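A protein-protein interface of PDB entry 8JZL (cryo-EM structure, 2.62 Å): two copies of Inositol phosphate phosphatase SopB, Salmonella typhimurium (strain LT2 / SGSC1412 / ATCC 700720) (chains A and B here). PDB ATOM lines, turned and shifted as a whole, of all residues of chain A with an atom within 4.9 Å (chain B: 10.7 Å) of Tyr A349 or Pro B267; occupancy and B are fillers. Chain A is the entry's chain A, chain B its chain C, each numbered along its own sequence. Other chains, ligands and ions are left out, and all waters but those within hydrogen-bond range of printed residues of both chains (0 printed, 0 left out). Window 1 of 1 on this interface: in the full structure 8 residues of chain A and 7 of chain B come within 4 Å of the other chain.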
ATOM      1  N   ARG A 333      13.794  -5.156 -14.477  1.00  0.00           N
ATOM      2  CA  ARG A 333      12.793  -6.195 -14.641  1.00  0.00           C
ATOM      3  C   ARG A 333      12.041  -6.415 -13.341  1.00  0.00           C
ATOM      4  O   ARG A 333      12.632  -6.333 -12.264  1.00  0.00           O
ATOM      5  CB  ARG A 333      13.443  -7.504 -15.074  1.00  0.00           C
ATOM      6  CG  ARG A 333      14.167  -7.402 -16.389  1.00  0.00           C
ATOM      7  CD  ARG A 333      15.218  -8.482 -16.520  1.00  0.00           C
ATOM      8  NE  ARG A 333      14.654  -9.733 -17.005  1.00  0.00           N
ATOM      9  CZ  ARG A 333      14.325  -9.958 -18.271  1.00  0.00           C
ATOM     10  NH1 ARG A 333      14.505  -9.013 -19.183  1.00  0.00           N
ATOM     11  NH2 ARG A 333      13.816 -11.129 -18.626  1.00  0.00           N
ATOM     12  N   PRO A 334      10.746  -6.698 -13.412  1.00  0.00           N
ATOM     13  CA  PRO A 334       9.953  -6.823 -12.190  1.00  0.00           C
ATOM     14  C   PRO A 334      10.401  -7.994 -11.336  1.00  0.00           C
ATOM     15  O   PRO A 334      10.832  -9.031 -11.838  1.00  0.00           O
ATOM     16  CB  PRO A 334       8.532  -7.036 -12.713  1.00  0.00           C
ATOM     17  CG  PRO A 334       8.563  -6.578 -14.111  1.00  0.00           C
ATOM     18  CD  PRO A 334       9.923  -6.860 -14.614  1.00  0.00           C
ATOM     19  N   LEU A 342       5.183 -13.757 -13.375  1.00  0.00           N
ATOM     20  CA  LEU A 342       5.680 -13.767 -14.742  1.00  0.00           C
ATOM     21  C   LEU A 342       6.551 -14.978 -15.015  1.00  0.00           C
ATOM     22  O   LEU A 342       6.668 -15.405 -16.164  1.00  0.00           O
ATOM     23  CB  LEU A 342       6.453 -12.491 -15.025  1.00  0.00           C
ATOM     24  CG  LEU A 342       5.589 -11.255 -15.211  1.00  0.00           C
ATOM     25  CD1 LEU A 342       6.450 -10.044 -15.394  1.00  0.00           C
ATOM     26  CD2 LEU A 342       4.692 -11.440 -16.391  1.00  0.00           C
ATOM     27  N   PRO A 346       2.763 -16.644 -18.365  1.00  0.00           N
ATOM     28  CA  PRO A 346       1.339 -16.628 -18.672  1.00  0.00           C
ATOM     29  C   PRO A 346       1.072 -15.833 -19.933  1.00  0.00           C
ATOM     30  O   PRO A 346       1.873 -15.005 -20.360  1.00  0.00           O
ATOM     31  CB  PRO A 346       0.746 -15.926 -17.460  1.00  0.00           C
ATOM     32  CG  PRO A 346       1.782 -14.938 -17.124  1.00  0.00           C
ATOM     33  CD  PRO A 346       3.112 -15.555 -17.444  1.00  0.00           C
ATOM     34  N   ASP A 347      -0.092 -16.069 -20.510  1.00  0.00           N
ATOM     35  CA  ASP A 347      -0.509 -15.313 -21.679  1.00  0.00           C
ATOM     36  C   ASP A 347      -1.007 -13.935 -21.324  1.00  0.00           C
ATOM     37  O   ASP A 347      -1.652 -13.274 -22.136  1.00  0.00           O
ATOM     38  CB  ASP A 347      -1.579 -16.090 -22.434  1.00  0.00           C
ATOM     39  CG  ASP A 347      -2.712 -16.487 -21.544  1.00  0.00           C
ATOM     40  OD1 ASP A 347      -2.613 -16.223 -20.330  1.00  0.00           O
ATOM     41  OD2 ASP A 347      -3.690 -17.072 -22.047  1.00  0.00           O
ATOM     42  N   ASN A 348      -0.706 -13.501 -20.110  1.00  0.00           N
ATOM     43  CA  ASN A 348      -1.147 -12.234 -19.559  1.00  0.00           C
ATOM     44  C   ASN A 348      -0.024 -11.214 -19.507  1.00  0.00           C
ATOM     45  O   ASN A 348      -0.214 -10.125 -18.971  1.00  0.00           O
ATOM     46  CB  ASN A 348      -1.691 -12.484 -18.158  1.00  0.00           C
ATOM     47  CG  ASN A 348      -2.571 -11.398 -17.685  1.00  0.00           C
ATOM     48  OD1 ASN A 348      -3.017 -10.570 -18.467  1.00  0.00           O
ATOM     49  ND2 ASN A 348      -2.842 -11.382 -16.392  1.00  0.00           N
ATOM     50  N   TYR A 349       1.136 -11.537 -20.074  1.00  0.00           N
ATOM     51  CA  TYR A 349       2.355 -10.800 -19.769  1.00  0.00           C
ATOM     52  C   TYR A 349       2.287  -9.354 -20.222  1.00  0.00           C
ATOM     53  O   TYR A 349       2.894  -8.482 -19.598  1.00  0.00           O
ATOM     54  CB  TYR A 349       3.546 -11.490 -20.416  1.00  0.00           C
ATOM     55  CG  TYR A 349       3.490 -11.459 -21.915  1.00  0.00           C
ATOM     56  CD1 TYR A 349       2.759 -12.394 -22.612  1.00  0.00           C
ATOM     57  CD2 TYR A 349       4.153 -10.485 -22.629  1.00  0.00           C
ATOM     58  CE1 TYR A 349       2.696 -12.364 -23.972  1.00  0.00           C
ATOM     59  CE2 TYR A 349       4.094 -10.447 -23.987  1.00  0.00           C
ATOM     60  CZ  TYR A 349       3.363 -11.387 -24.654  1.00  0.00           C
ATOM     61  OH  TYR A 349       3.303 -11.354 -26.022  1.00  0.00           O
ATOM     62  N   GLU A 350       1.575  -9.081 -21.309  1.00  0.00           N
ATOM     63  CA  GLU A 350       1.564  -7.734 -21.864  1.00  0.00           C
ATOM     64  C   GLU A 350       0.990  -6.734 -20.875  1.00  0.00           C
ATOM     65  O   GLU A 350       1.609  -5.704 -20.579  1.00  0.00           O
ATOM     66  CB  GLU A 350       0.763  -7.729 -23.159  1.00  0.00           C
ATOM     67  CG  GLU A 350       0.834  -6.437 -23.923  1.00  0.00           C
ATOM     68  CD  GLU A 350       2.218  -6.145 -24.433  1.00  0.00           C
ATOM     69  OE1 GLU A 350       3.010  -5.537 -23.687  1.00  0.00           O
ATOM     70  OE2 GLU A 350       2.517  -6.528 -25.581  1.00  0.00           O
ATOM     71  N   VAL A 351      -0.193  -7.026 -20.343  1.00  0.00           N
ATOM     72  CA  VAL A 351      -0.849  -6.099 -19.433  1.00  0.00           C
ATOM     73  C   VAL A 351      -0.038  -5.938 -18.161  1.00  0.00           C
ATOM     74  O   VAL A 351       0.110  -4.829 -17.638  1.00  0.00           O
ATOM     75  CB  VAL A 351      -2.272  -6.584 -19.128  1.00  0.00           C
ATOM     76  CG1 VAL A 351      -2.948  -5.629 -18.197  1.00  0.00           C
ATOM     77  CG2 VAL A 351      -3.049  -6.724 -20.403  1.00  0.00           C
ATOM     78  N   VAL A 352       0.495  -7.038 -17.639  1.00  0.00           N
ATOM     79  CA  VAL A 352       1.229  -6.983 -16.384  1.00  0.00           C
ATOM     80  C   VAL A 352       2.460  -6.108 -16.525  1.00  0.00           C
ATOM     81  O   VAL A 352       2.757  -5.287 -15.652  1.00  0.00           O
ATOM     82  CB  VAL A 352       1.597  -8.399 -15.924  1.00  0.00           C
ATOM     83  CG1 VAL A 352       2.521  -8.333 -14.756  1.00  0.00           C
ATOM     84  CG2 VAL A 352       0.359  -9.150 -15.555  1.00  0.00           C
ATOM     85  N   ASN A 353       3.197  -6.263 -17.620  1.00  0.00           N
ATOM     86  CA  ASN A 353       4.397  -5.462 -17.804  1.00  0.00           C
ATOM     87  C   ASN A 353       4.065  -3.985 -17.903  1.00  0.00           C
ATOM     88  O   ASN A 353       4.765  -3.144 -17.330  1.00  0.00           O
ATOM     89  CB  ASN A 353       5.142  -5.925 -19.045  1.00  0.00           C
ATOM     90  CG  ASN A 353       6.035  -7.090 -18.771  1.00  0.00           C
ATOM     91  OD1 ASN A 353       6.962  -6.994 -17.978  1.00  0.00           O
ATOM     92  ND2 ASN A 353       5.764  -8.207 -19.419  1.00  0.00           N
ATOM     93  N   TRP B 261      17.822  -7.836 -28.613  1.00  0.00           N
ATOM     94  CA  TRP B 261      17.866  -8.804 -27.527  1.00  0.00           C
ATOM     95  C   TRP B 261      16.785  -8.515 -26.500  1.00  0.00           C
ATOM     96  O   TRP B 261      16.142  -9.437 -25.989  1.00  0.00           O
ATOM     97  CB  TRP B 261      19.236  -8.799 -26.863  1.00  0.00           C
ATOM     98  CG  TRP B 261      20.307  -9.489 -27.627  1.00  0.00           C
ATOM     99  CD1 TRP B 261      21.556  -9.027 -27.843  1.00  0.00           C
ATOM    100  CD2 TRP B 261      20.240 -10.768 -28.262  1.00  0.00           C
ATOM    101  NE1 TRP B 261      22.275  -9.924 -28.576  1.00  0.00           N
ATOM    102  CE2 TRP B 261      21.487 -11.004 -28.845  1.00  0.00           C
ATOM    103  CE3 TRP B 261      19.248 -11.733 -28.393  1.00  0.00           C
ATOM    104  CZ2 TRP B 261      21.768 -12.156 -29.546  1.00  0.00           C
ATOM    105  CZ3 TRP B 261      19.530 -12.872 -29.090  1.00  0.00           C
ATOM    106  CH2 TRP B 261      20.777 -13.078 -29.658  1.00  0.00           C
ATOM    107  N   GLN B 262      16.564  -7.241 -26.189  1.00  0.00           N
ATOM    108  CA  GLN B 262      15.533  -6.898 -25.219  1.00  0.00           C
ATOM    109  C   GLN B 262      14.162  -7.339 -25.692  1.00  0.00           C
ATOM    110  O   GLN B 262      13.355  -7.832 -24.901  1.00  0.00           O
ATOM    111  CB  GLN B 262      15.530  -5.403 -24.956  1.00  0.00           C
ATOM    112  CG  GLN B 262      16.380  -4.987 -23.802  1.00  0.00           C
ATOM    113  CD  GLN B 262      16.544  -3.494 -23.750  1.00  0.00           C
ATOM    114  OE1 GLN B 262      15.655  -2.750 -24.161  1.00  0.00           O
ATOM    115  NE2 GLN B 262      17.687  -3.039 -23.257  1.00  0.00           N
ATOM    116  N   SER B 263      13.871  -7.161 -26.975  1.00  0.00           N
ATOM    117  CA  SER B 263      12.556  -7.538 -27.466  1.00  0.00           C
ATOM    118  C   SER B 263      12.331  -9.036 -27.435  1.00  0.00           C
ATOM    119  O   SER B 263      11.180  -9.468 -27.359  1.00  0.00           O
ATOM    120  CB  SER B 263      12.351  -7.028 -28.879  1.00  0.00           C
ATOM    121  OG  SER B 263      12.267  -5.620 -28.891  1.00  0.00           O
ATOM    122  N   LEU B 264      13.381  -9.839 -27.506  1.00  0.00           N
ATOM    123  CA  LEU B 264      13.175 -11.274 -27.402  1.00  0.00           C
ATOM    124  C   LEU B 264      13.125 -11.775 -25.972  1.00  0.00           C
ATOM    125  O   LEU B 264      12.572 -12.849 -25.734  1.00  0.00           O
ATOM    126  CB  LEU B 264      14.260 -12.035 -28.148  1.00  0.00           C
ATOM    127  CG  LEU B 264      14.211 -11.880 -29.656  1.00  0.00           C
ATOM    128  CD1 LEU B 264      15.385 -12.587 -30.248  1.00  0.00           C
ATOM    129  CD2 LEU B 264      12.935 -12.456 -30.183  1.00  0.00           C
ATOM    130  N   THR B 265      13.679 -11.043 -25.017  1.00  0.00           N
ATOM    131  CA  THR B 265      13.684 -11.474 -23.626  1.00  0.00           C
ATOM    132  C   THR B 265      12.752 -10.627 -22.773  1.00  0.00           C
ATOM    133  O   THR B 265      13.053 -10.306 -21.626  1.00  0.00           O
ATOM    134  CB  THR B 265      15.092 -11.443 -23.051  1.00  0.00           C
ATOM    135  OG1 THR B 265      15.508 -10.086 -22.888  1.00  0.00           O
ATOM    136  CG2 THR B 265      16.042 -12.140 -23.978  1.00  0.00           C
ATOM    137  N   GLN B 266      11.621 -10.248 -23.328  1.00  0.00           N
ATOM    138  CA  GLN B 266      10.614  -9.550 -22.552  1.00  0.00           C
ATOM    139  C   GLN B 266      10.049 -10.494 -21.501  1.00  0.00           C
ATOM    140  O   GLN B 266       9.723 -11.637 -21.823  1.00  0.00           O
ATOM    141  CB  GLN B 266       9.518  -9.054 -23.473  1.00  0.00           C
ATOM    142  CG  GLN B 266       8.393  -8.365 -22.779  1.00  0.00           C
ATOM    143  CD  GLN B 266       7.602  -7.503 -23.722  1.00  0.00           C
ATOM    144  OE1 GLN B 266       7.724  -7.629 -24.939  1.00  0.00           O
ATOM    145  NE2 GLN B 266       6.772  -6.629 -23.172  1.00  0.00           N
ATOM    146  N   PRO B 267       9.936 -10.070 -20.246  1.00  0.00           N
ATOM    147  CA  PRO B 267       9.583 -11.013 -19.179  1.00  0.00           C
ATOM    148  C   PRO B 267       8.223 -11.647 -19.402  1.00  0.00           C
ATOM    149  O   PRO B 267       7.266 -10.983 -19.792  1.00  0.00           O
ATOM    150  CB  PRO B 267       9.591 -10.140 -17.925  1.00  0.00           C
ATOM    151  CG  PRO B 267      10.416  -8.978 -18.279  1.00  0.00           C
ATOM    152  CD  PRO B 267      10.191  -8.726 -19.721  1.00  0.00           C
ATOM    153  N   GLY B 268       8.142 -12.945 -19.143  1.00  0.00           N
ATOM    154  CA  GLY B 268       6.909 -13.673 -19.323  1.00  0.00           C
ATOM    155  C   GLY B 268       6.520 -13.932 -20.757  1.00  0.00           C
ATOM    156  O   GLY B 268       5.476 -14.541 -20.995  1.00  0.00           O
ATOM    157  N   LYS B 269       7.327 -13.506 -21.715  1.00  0.00           N
ATOM    158  CA  LYS B 269       7.018 -13.652 -23.129  1.00  0.00           C
ATOM    159  C   LYS B 269       7.682 -14.914 -23.652  1.00  0.00           C
ATOM    160  O   LYS B 269       8.907 -15.040 -23.593  1.00  0.00           O
ATOM    161  CB  LYS B 269       7.514 -12.427 -23.888  1.00  0.00           C
ATOM    162  CG  LYS B 269       7.595 -12.567 -25.382  1.00  0.00           C
ATOM    163  CD  LYS B 269       6.242 -12.518 -26.015  1.00  0.00           C
ATOM    164  CE  LYS B 269       6.363 -12.409 -27.512  1.00  0.00           C
ATOM    165  NZ  LYS B 269       6.995 -11.123 -27.884  1.00  0.00           N
ATOM    166  N   MET B 270       6.888 -15.843 -24.158  1.00  0.00           N
ATOM    167  CA  MET B 270       7.427 -17.084 -24.686  1.00  0.00           C
ATOM    168  C   MET B 270       7.608 -16.981 -26.191  1.00  0.00           C
ATOM    169  O   MET B 270       6.732 -16.488 -26.899  1.00  0.00           O
ATOM    170  CB  MET B 270       6.525 -18.262 -24.344  1.00  0.00           C
ATOM    171  CG  MET B 270       7.108 -19.576 -24.767  1.00  0.00           C
ATOM    172  SD  MET B 270       6.064 -20.963 -24.352  1.00  0.00           S
ATOM    173  CE  MET B 270       6.294 -20.996 -22.584  1.00  0.00           C
ATOM    174  N   ILE B 271       8.752 -17.450 -26.671  1.00  0.00           N
ATOM    175  CA  ILE B 271       9.181 -17.244 -28.047  1.00  0.00           C
ATOM    176  C   ILE B 271       8.856 -18.474 -28.875  1.00  0.00           C
ATOM    177  O   ILE B 271       9.052 -19.607 -28.427  1.00  0.00           O
ATOM    178  CB  ILE B 271      10.682 -16.929 -28.106  1.00  0.00           C
ATOM    179  CG1 ILE B 271      10.964 -15.645 -27.347  1.00  0.00           C
ATOM    180  CG2 ILE B 271      11.132 -16.772 -29.523  1.00  0.00           C
ATOM    181  CD1 ILE B 271      10.073 -14.518 -27.747  1.00  0.00           C
ATOM    182  N   HIS B 272       8.355 -18.253 -30.083  1.00  0.00           N
ATOM    183  CA  HIS B 272       8.022 -19.323 -31.009  1.00  0.00           C
ATOM    184  C   HIS B 272       8.994 -19.308 -32.175  1.00  0.00           C
ATOM    185  O   HIS B 272       9.170 -18.276 -32.826  1.00  0.00           O
ATOM    186  CB  HIS B 272       6.593 -19.166 -31.516  1.00  0.00           C
ATOM    187  CG  HIS B 272       5.560 -19.364 -30.458  1.00  0.00           C
ATOM    188  ND1 HIS B 272       4.235 -19.046 -30.645  1.00  0.00           N
ATOM    189  CD2 HIS B 272       5.657 -19.855 -29.203  1.00  0.00           C
ATOM    190  CE1 HIS B 272       3.559 -19.328 -29.547  1.00  0.00           C
ATOM    191  NE2 HIS B 272       4.399 -19.822 -28.657  1.00  0.00           N
ATOM    192  N   ILE B 287      10.395 -21.599 -26.831  1.00  0.00           N
ATOM    193  CA  ILE B 287      11.649 -21.339 -26.143  1.00  0.00           C
ATOM    194  C   ILE B 287      11.415 -20.303 -25.058  1.00  0.00           C
ATOM    195  O   ILE B 287      10.651 -19.353 -25.249  1.00  0.00           O
ATOM    196  CB  ILE B 287      12.732 -20.852 -27.121  1.00  0.00           C
ATOM    197  CG1 ILE B 287      12.885 -21.842 -28.257  1.00  0.00           C
ATOM    198  CG2 ILE B 287      14.048 -20.706 -26.425  1.00  0.00           C
ATOM    199  CD1 ILE B 287      13.456 -23.138 -27.809  1.00  0.00           C
ATOM    200  N   LYS B 288      12.069 -20.493 -23.927  1.00  0.00           N
ATOM    201  CA  LYS B 288      12.128 -19.503 -22.866  1.00  0.00           C
ATOM    202  C   LYS B 288      13.541 -18.940 -22.819  1.00  0.00           C
ATOM    203  O   LYS B 288      14.403 -19.474 -22.113  1.00  0.00           O
ATOM    204  CB  LYS B 288      11.735 -20.126 -21.533  1.00  0.00           C
ATOM    205  CG  LYS B 288      10.253 -20.358 -21.408  1.00  0.00           C
ATOM    206  CD  LYS B 288       9.934 -21.751 -20.940  1.00  0.00           C
ATOM    207  CE  LYS B 288      10.250 -21.922 -19.481  1.00  0.00           C
ATOM    208  NZ  LYS B 288       9.801 -23.247 -18.990  1.00  0.00           N
ATOM    209  N   PRO B 289      13.822 -17.890 -23.578  1.00  0.00           N
ATOM    210  CA  PRO B 289      15.198 -17.422 -23.714  1.00  0.00           C
ATOM    211  C   PRO B 289      15.657 -16.663 -22.490  1.00  0.00           C
ATOM    212  O   PRO B 289      14.865 -16.184 -21.681  1.00  0.00           O
ATOM    213  CB  PRO B 289      15.138 -16.496 -24.928  1.00  0.00           C
ATOM    214  CG  PRO B 289      13.890 -16.841 -25.612  1.00  0.00           C
ATOM    215  CD  PRO B 289      12.940 -17.225 -24.539  1.00  0.00           C
ATOM    216  N   ASP B 290      16.972 -16.544 -22.375  1.00  0.00           N
ATOM    217  CA  ASP B 290      17.581 -15.743 -21.324  1.00  0.00           C
ATOM    218  C   ASP B 290      18.940 -15.300 -21.831  1.00  0.00           C
ATOM    219  O   ASP B 290      19.850 -16.120 -21.941  1.00  0.00           O
ATOM    220  CB  ASP B 290      17.707 -16.539 -20.041  1.00  0.00           C
ATOM    221  CG  ASP B 290      17.503 -15.694 -18.826  1.00  0.00           C
ATOM    222  OD1 ASP B 290      17.371 -14.465 -18.983  1.00  0.00           O
ATOM    223  OD2 ASP B 290      17.467 -16.251 -17.713  1.00  0.00           O
ATOM    224  N   VAL B 291      19.081 -14.018 -22.139  1.00  0.00           N
ATOM    225  CA  VAL B 291      20.254 -13.510 -22.830  1.00  0.00           C
ATOM    226  C   VAL B 291      20.945 -12.484 -21.953  1.00  0.00           C
ATOM    227  O   VAL B 291      20.292 -11.590 -21.408  1.00  0.00           O
ATOM    228  CB  VAL B 291      19.882 -12.893 -24.183  1.00  0.00           C
ATOM    229  CG1 VAL B 291      21.106 -12.377 -24.859  1.00  0.00           C
ATOM    230  CG2 VAL B 291      19.205 -13.914 -25.043  1.00  0.00           C
ATOM    231  N   GLN B 322      23.246  -9.849 -14.134  1.00  0.00           N
ATOM    232  CA  GLN B 322      22.512 -11.022 -14.576  1.00  0.00           C
ATOM    233  C   GLN B 322      23.352 -12.281 -14.480  1.00  0.00           C
ATOM    234  O   GLN B 322      22.815 -13.364 -14.248  1.00  0.00           O
ATOM    235  CB  GLN B 322      22.050 -10.803 -16.004  1.00  0.00           C
ATOM    236  CG  GLN B 322      20.905 -11.639 -16.428  1.00  0.00           C
ATOM    237  CD  GLN B 322      20.262 -11.082 -17.657  1.00  0.00           C
ATOM    238  OE1 GLN B 322      20.721 -10.086 -18.203  1.00  0.00           O
ATOM    239  NE2 GLN B 322      19.200 -11.721 -18.111  1.00  0.00           N
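The guanidinium group (NH1) of Arg A333 sits at hydrogen-bond distance from the backbone carbonyl oxygen (O) of Thr B265 (3.1 Å).
The backbone carbonyl oxygen of Pro B267 sits at hydrogen-bond distance from the side-chain amide nitrogen of Asn A353 (3.2 Å).
The backbone carbonyl oxygen (O) of Tyr A349 sits at hydrogen-bond distance from the side-chain amide nitrogen (ND2) of Asn A353 (2.9 Å).
The backbone carbonyl oxygen (O) of Trp B261 is in hydrogen-bond range of the side-chain hydroxyl (OG1) of Thr B265 (3.2 Å).
O of Leu A342 touches CA of Gly B268 (3.6 Å).
Pro A346 touches Gly B268.
O of Pro B267 touches CB of Tyr A349, 3.8 Å away.
CB of Tyr A349 touches O of Gly B268 (3.7 Å).
Tyr A349 touches Lys B269 (OH to CD, 3.2 Å).
Glu A350 touches Gln B266.
Of chain B, only Pro B267, Gly B268 and Lys B269 come within 4 Å of Tyr A349.
Of chain A, only Tyr A349 and Asn A353 come within 4 Å of Pro B267.
Pro A346 touches just one residue of chain B: Gly B268 (3.7 Å).
Of chain B, only Gln B266 (3.95 Å) comes within 4 Å of Glu A350.
No residue of chain B comes within 4 Å of Val A352.
Of chain B, only Pro B267 comes within 4 Å of Asn A353.
Printed residues of chain B within 4 Å of Arg A333: Thr B265 (3.1 Å).
Of the printed residues of chain A, Gly B268 touches Leu A342 (3.6 Å), Pro A346 (3.7 Å) and Tyr A349 (3.7 Å).
Of the printed residues of chain A, Gln B266 touches Glu A350.
Printed residues of chain B within 4 Å of Leu A342: Gly B268 (3.6 Å).
Of the printed residues of chain A, Thr B265 touches Arg A333.
Lys B288 touches none of the printed residues of chain A.
The nearest residue of chain B that does not touch Tyr A349 is Gln B266 (4.6 Å).
Of the 18 printed residues of chain B, 5 touch a printed residue of chain A.
Among the printed residues, 8 pairs touch across the chains.
Among the printed residues, no Asp or Glu carboxylate lies within 4 Å of a Lys or Arg side-chain nitrogen of the other chain.
No position is printed for both chains.
Of the 8 pairs that touch across the chains among the printed residues, none has its exchanged pair printed and touching as well.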
